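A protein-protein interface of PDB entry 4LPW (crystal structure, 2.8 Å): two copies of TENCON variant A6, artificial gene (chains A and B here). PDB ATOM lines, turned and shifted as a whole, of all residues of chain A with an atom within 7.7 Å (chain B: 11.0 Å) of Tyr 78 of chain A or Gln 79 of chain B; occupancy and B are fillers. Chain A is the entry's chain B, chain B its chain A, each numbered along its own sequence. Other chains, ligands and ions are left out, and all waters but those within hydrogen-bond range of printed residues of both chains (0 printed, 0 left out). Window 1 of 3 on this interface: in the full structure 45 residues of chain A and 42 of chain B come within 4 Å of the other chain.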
ATOM      1  N   LEU A   2     -32.347  19.226 -19.019  1.00  0.00           N
ATOM      2  CA  LEU A   2     -33.226  19.916 -19.959  1.00  0.00           C
ATOM      3  C   LEU A   2     -34.301  20.732 -19.207  1.00  0.00           C
ATOM      4  O   LEU A   2     -34.917  20.242 -18.246  1.00  0.00           O
ATOM      5  CB  LEU A   2     -33.881  18.909 -20.936  1.00  0.00           C
ATOM      6  CG  LEU A   2     -33.034  18.340 -22.086  1.00  0.00           C
ATOM      7  CD1 LEU A   2     -33.491  16.950 -22.558  1.00  0.00           C
ATOM      8  CD2 LEU A   2     -33.006  19.305 -23.258  1.00  0.00           C
ATOM      9  N   ASP A  30     -35.304  17.221 -29.492  1.00  0.00           N
ATOM     10  CA  ASP A  30     -35.241  16.594 -30.801  1.00  0.00           C
ATOM     11  C   ASP A  30     -36.637  16.127 -31.110  1.00  0.00           C
ATOM     12  O   ASP A  30     -37.029  16.027 -32.270  1.00  0.00           O
ATOM     13  CB  ASP A  30     -34.316  15.373 -30.741  1.00  0.00           C
ATOM     14  CG  ASP A  30     -33.819  14.930 -32.106  1.00  0.00           C
ATOM     15  OD1 ASP A  30     -33.418  15.806 -32.903  1.00  0.00           O
ATOM     16  OD2 ASP A  30     -33.816  13.705 -32.383  1.00  0.00           O
ATOM     17  N   VAL A  75     -37.631  15.550 -25.191  1.00  0.00           N
ATOM     18  CA  VAL A  75     -36.558  14.576 -25.389  1.00  0.00           C
ATOM     19  C   VAL A  75     -35.380  15.156 -26.156  1.00  0.00           C
ATOM     20  O   VAL A  75     -35.550  16.026 -27.006  1.00  0.00           O
ATOM     21  CB  VAL A  75     -37.049  13.356 -26.210  1.00  0.00           C
ATOM     22  CG1 VAL A  75     -36.033  12.242 -26.174  1.00  0.00           C
ATOM     23  CG2 VAL A  75     -38.382  12.866 -25.696  1.00  0.00           C
ATOM     24  N   PHE A  76     -34.182  14.654 -25.867  1.00  0.00           N
ATOM     25  CA  PHE A  76     -33.084  14.730 -26.827  1.00  0.00           C
ATOM     26  C   PHE A  76     -32.248  13.435 -26.895  1.00  0.00           C
ATOM     27  O   PHE A  76     -31.602  13.072 -25.909  1.00  0.00           O
ATOM     28  CB  PHE A  76     -32.194  15.918 -26.515  1.00  0.00           C
ATOM     29  CG  PHE A  76     -31.352  16.363 -27.681  1.00  0.00           C
ATOM     30  CD1 PHE A  76     -30.546  15.472 -28.357  1.00  0.00           C
ATOM     31  CD2 PHE A  76     -31.394  17.668 -28.117  1.00  0.00           C
ATOM     32  CE1 PHE A  76     -29.780  15.863 -29.408  1.00  0.00           C
ATOM     33  CE2 PHE A  76     -30.634  18.068 -29.182  1.00  0.00           C
ATOM     34  CZ  PHE A  76     -29.822  17.159 -29.827  1.00  0.00           C
ATOM     35  N   PRO A  77     -32.281  12.720 -28.048  1.00  0.00           N
ATOM     36  CA  PRO A  77     -31.290  11.648 -28.269  1.00  0.00           C
ATOM     37  C   PRO A  77     -29.907  12.221 -28.582  1.00  0.00           C
ATOM     38  O   PRO A  77     -29.449  12.168 -29.726  1.00  0.00           O
ATOM     39  CB  PRO A  77     -31.847  10.883 -29.481  1.00  0.00           C
ATOM     40  CG  PRO A  77     -33.316  11.153 -29.443  1.00  0.00           C
ATOM     41  CD  PRO A  77     -33.437  12.579 -28.953  1.00  0.00           C
ATOM     42  N   TYR A  78     -29.245  12.740 -27.554  1.00  0.00           N
ATOM     43  CA  TYR A  78     -28.057  13.563 -27.746  1.00  0.00           C
ATOM     44  C   TYR A  78     -26.774  12.808 -28.035  1.00  0.00           C
ATOM     45  O   TYR A  78     -26.596  12.243 -29.115  1.00  0.00           O
ATOM     46  CB  TYR A  78     -27.868  14.500 -26.546  1.00  0.00           C
ATOM     47  N   GLN A  79     -25.898  12.837 -27.035  1.00  0.00           N
ATOM     48  CA  GLN A  79     -24.523  12.376 -27.103  1.00  0.00           C
ATOM     49  C   GLN A  79     -24.259  11.027 -27.780  1.00  0.00           C
ATOM     50  O   GLN A  79     -24.570   9.966 -27.231  1.00  0.00           O
ATOM     51  CB  GLN A  79     -23.945  12.354 -25.696  1.00  0.00           C
ATOM     52  N   TYR A  80     -23.670  11.078 -28.971  1.00  0.00           N
ATOM     53  CA  TYR A  80     -22.959   9.933 -29.520  1.00  0.00           C
ATOM     54  C   TYR A  80     -21.494  10.099 -29.108  1.00  0.00           C
ATOM     55  O   TYR A  80     -21.044  11.214 -28.837  1.00  0.00           O
ATOM     56  CB  TYR A  80     -23.025   9.931 -31.053  1.00  0.00           C
ATOM     57  CG  TYR A  80     -24.291   9.386 -31.659  1.00  0.00           C
ATOM     58  CD1 TYR A  80     -24.415   8.034 -31.955  1.00  0.00           C
ATOM     59  CD2 TYR A  80     -25.352  10.220 -31.964  1.00  0.00           C
ATOM     60  CE1 TYR A  80     -25.571   7.522 -32.528  1.00  0.00           C
ATOM     61  CE2 TYR A  80     -26.515   9.717 -32.534  1.00  0.00           C
ATOM     62  CZ  TYR A  80     -26.618   8.366 -32.814  1.00  0.00           C
ATOM     63  OH  TYR A  80     -27.768   7.859 -33.379  1.00  0.00           O
ATOM     64  N   THR A  81     -20.746   9.006 -29.083  1.00  0.00           N
ATOM     65  CA  THR A  81     -19.294   9.116 -29.140  1.00  0.00           C
ATOM     66  C   THR A  81     -18.734   8.124 -30.154  1.00  0.00           C
ATOM     67  O   THR A  81     -19.175   6.971 -30.206  1.00  0.00           O
ATOM     68  CB  THR A  81     -18.632   8.937 -27.753  1.00  0.00           C
ATOM     69  OG1 THR A  81     -18.807  10.137 -26.992  1.00  0.00           O
ATOM     70  CG2 THR A  81     -17.140   8.682 -27.890  1.00  0.00           C
ATOM     71  N   LEU B   2     -13.461   4.906 -25.812  1.00  0.00           N
ATOM     72  CA  LEU B   2     -13.648   3.922 -26.884  1.00  0.00           C
ATOM     73  C   LEU B   2     -12.339   3.606 -27.639  1.00  0.00           C
ATOM     74  O   LEU B   2     -11.875   4.395 -28.476  1.00  0.00           O
ATOM     75  CB  LEU B   2     -14.747   4.373 -27.871  1.00  0.00           C
ATOM     76  CG  LEU B   2     -16.210   4.268 -27.423  1.00  0.00           C
ATOM     77  CD1 LEU B   2     -17.139   5.000 -28.374  1.00  0.00           C
ATOM     78  CD2 LEU B   2     -16.646   2.819 -27.278  1.00  0.00           C
ATOM     79  N   ASP B  30     -22.077  -0.117 -30.741  1.00  0.00           N
ATOM     80  CA  ASP B  30     -23.462  -0.391 -31.099  1.00  0.00           C
ATOM     81  C   ASP B  30     -23.594  -0.344 -32.606  1.00  0.00           C
ATOM     82  O   ASP B  30     -24.397  -1.063 -33.209  1.00  0.00           O
ATOM     83  CB  ASP B  30     -24.420   0.621 -30.450  1.00  0.00           C
ATOM     84  CG  ASP B  30     -24.985   0.131 -29.102  1.00  0.00           C
ATOM     85  OD1 ASP B  30     -25.899  -0.722 -29.104  1.00  0.00           O
ATOM     86  OD2 ASP B  30     -24.529   0.607 -28.037  1.00  0.00           O
ATOM     87  N   VAL B  75     -18.883   3.378 -33.201  1.00  0.00           N
ATOM     88  CA  VAL B  75     -19.832   4.235 -32.495  1.00  0.00           C
ATOM     89  C   VAL B  75     -20.375   3.574 -31.226  1.00  0.00           C
ATOM     90  O   VAL B  75     -20.578   2.359 -31.189  1.00  0.00           O
ATOM     91  CB  VAL B  75     -21.041   4.565 -33.386  1.00  0.00           C
ATOM     92  CG1 VAL B  75     -21.750   5.790 -32.867  1.00  0.00           C
ATOM     93  CG2 VAL B  75     -20.596   4.764 -34.818  1.00  0.00           C
ATOM     94  N   PHE B  76     -20.646   4.378 -30.200  1.00  0.00           N
ATOM     95  CA  PHE B  76     -21.319   3.876 -28.997  1.00  0.00           C
ATOM     96  C   PHE B  76     -22.169   4.898 -28.231  1.00  0.00           C
ATOM     97  O   PHE B  76     -21.621   5.755 -27.527  1.00  0.00           O
ATOM     98  CB  PHE B  76     -20.310   3.280 -28.031  1.00  0.00           C
ATOM     99  CG  PHE B  76     -20.948   2.629 -26.854  1.00  0.00           C
ATOM    100  CD1 PHE B  76     -21.451   1.353 -26.961  1.00  0.00           C
ATOM    101  CD2 PHE B  76     -21.080   3.302 -25.652  1.00  0.00           C
ATOM    102  CE1 PHE B  76     -22.058   0.741 -25.888  1.00  0.00           C
ATOM    103  CE2 PHE B  76     -21.684   2.698 -24.568  1.00  0.00           C
ATOM    104  CZ  PHE B  76     -22.177   1.413 -24.685  1.00  0.00           C
ATOM    105  N   PRO B  77     -23.512   4.775 -28.308  1.00  0.00           N
ATOM    106  CA  PRO B  77     -24.367   5.810 -27.713  1.00  0.00           C
ATOM    107  C   PRO B  77     -24.429   5.623 -26.209  1.00  0.00           C
ATOM    108  O   PRO B  77     -24.052   4.559 -25.721  1.00  0.00           O
ATOM    109  CB  PRO B  77     -25.742   5.523 -28.332  1.00  0.00           C
ATOM    110  CG  PRO B  77     -25.752   4.033 -28.453  1.00  0.00           C
ATOM    111  CD  PRO B  77     -24.307   3.617 -28.756  1.00  0.00           C
ATOM    112  N   TYR B  78     -24.882   6.645 -25.491  1.00  0.00           N
ATOM    113  CA  TYR B  78     -25.228   6.494 -24.084  1.00  0.00           C
ATOM    114  C   TYR B  78     -26.441   7.351 -23.796  1.00  0.00           C
ATOM    115  O   TYR B  78     -27.575   6.938 -24.021  1.00  0.00           O
ATOM    116  CB  TYR B  78     -24.064   6.890 -23.171  1.00  0.00           C
ATOM    117  N   GLN B  79     -26.185   8.562 -23.323  1.00  0.00           N
ATOM    118  CA  GLN B  79     -27.250   9.489 -22.977  1.00  0.00           C
ATOM    119  C   GLN B  79     -28.287   9.757 -24.075  1.00  0.00           C
ATOM    120  O   GLN B  79     -27.996  10.365 -25.102  1.00  0.00           O
ATOM    121  CB  GLN B  79     -26.667  10.819 -22.468  1.00  0.00           C
ATOM    122  N   TYR B  80     -29.495   9.258 -23.838  1.00  0.00           N
ATOM    123  CA  TYR B  80     -30.707   9.923 -24.279  1.00  0.00           C
ATOM    124  C   TYR B  80     -31.314  10.383 -22.955  1.00  0.00           C
ATOM    125  O   TYR B  80     -31.418   9.595 -22.014  1.00  0.00           O
ATOM    126  CB  TYR B  80     -31.638   8.961 -25.000  1.00  0.00           C
ATOM    127  N   THR B  81     -31.669  11.660 -22.851  1.00  0.00           N
ATOM    128  CA  THR B  81     -32.228  12.184 -21.609  1.00  0.00           C
ATOM    129  C   THR B  81     -33.538  12.903 -21.860  1.00  0.00           C
ATOM    130  O   THR B  81     -33.640  13.674 -22.802  1.00  0.00           O
ATOM    131  CB  THR B  81     -31.230  13.135 -20.918  1.00  0.00           C
ATOM    132  OG1 THR B  81     -30.384  12.376 -20.049  1.00  0.00           O
ATOM    133  CG2 THR B  81     -31.950  14.209 -20.099  1.00  0.00           C
ATOM    134  N   MET B  82     -34.541  12.666 -21.023  1.00  0.00           N
ATOM    135  CA  MET B  82     -35.811  13.362 -21.185  1.00  0.00           C
ATOM    136  C   MET B  82     -36.109  14.368 -20.077  1.00  0.00           C
ATOM    137  O   MET B  82     -35.408  14.450 -19.082  1.00  0.00           O
ATOM    138  CB  MET B  82     -36.953  12.360 -21.309  1.00  0.00           C
ATOM    139  CG  MET B  82     -36.862  11.496 -22.553  1.00  0.00           C
ATOM    140  SD  MET B  82     -38.189  10.289 -22.588  1.00  0.00           S
ATOM    141  CE  MET B  82     -38.333   9.933 -20.826  1.00  0.00           C
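O of Thr 81 of chain A is in hydrogen-bond range of N of Phe 76 of chain B, at 3.0 Å. The backbone NH of Phe 76 of chain A sits at hydrogen-bond distance from the backbone carbonyl oxygen of Thr 81 of chain B (3.3 Å).
Leu 2 of chain A touches Thr 81 of chain B, and with the chains exchanged Thr 81 of chain A touches Leu 2 of chain B. Tyr 78 of chain A touches Gln 79 of chain B, and with the chains exchanged Gln 79 of chain A touches Tyr 78 of chain B. Tyr 80 of chain A touches Val 75 of chain B, but with the chains exchanged Val 75 of chain A does not touch Tyr 80 of chain B (5.6 Å). Thr 81 of chain A touches Val 75 of chain B, but with the chains exchanged Val 75 of chain A does not touch Thr 81 of chain B (4.003 Å). Positions printed for both chains: 2, 30, 75, 76, 77, 78, 79, 80 and 81. Of the 11 pairs that touch across the chains among the printed residues, 7 have their exchanged pair printed and touching as well.
Printed residues of chain B within 4 Å of Val 75 of chain A: Met 82 (3.8 Å). Of chain B, only Tyr 80 (3.7 Å) and Thr 81 (3.3 Å) come within 4 Å of Phe 76 of chain A. Of chain B, only Gln 79 (3.6 Å) comes within 4 Å of Tyr 78 of chain A. Of the printed residues of chain A, Val 75 of chain B touches Tyr 80 (3.6 Å) and Thr 81 (3.6 Å). Tyr 78 of chain B touches just one residue of chain A: Gln 79. Of chain A, only Tyr 78 and Gln 79 come within 4 Å of Gln 79 of chain B. Of the printed residues of chain A, Thr 81 of chain B touches Leu 2 (3.3 Å) and Phe 76 (3.3 Å). Printed residues of chain A within 4 Å of Met 82 of chain B: Val 75 (3.8 Å).
The backbone NH (N) of Asp 30 of chain A is in hydrogen-bond range of the backbone carbonyl oxygen (O) of Val 75 of chain A, 2.8 Å away. The backbone NH (N) of Asp 30 of chain B is in hydrogen-bond range of the backbone carbonyl oxygen (O) of Val 75 of chain B (2.9 Å).
Among the printed residues, merely in contact across the chains: Leu 2 of chain A with Thr 81 of chain B (3.3 Å), Thr 81 of chain A with Leu 2 of chain B (3.4 Å), Tyr 80 of chain A with Val 75 of chain B (3.6 Å), Thr 81 of chain A with Val 75 of chain B (3.6 Å), Tyr 78 of chain A with Gln 79 of chain B (3.6 Å), Phe 76 of chain A with Tyr 80 of chain B (3.7 Å), Val 75 of chain A with Met 82 of chain B (3.8 Å), Gln 79 of chain A with Tyr 78 of chain B (3.8 Å) and Gln 79 of chain A with Gln 79 of chain B (3.8 Å).
Hydrophobic or aromatic side chains of chain B that line the printed part of chain A: Leu 2, Val 75 and Met 82.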
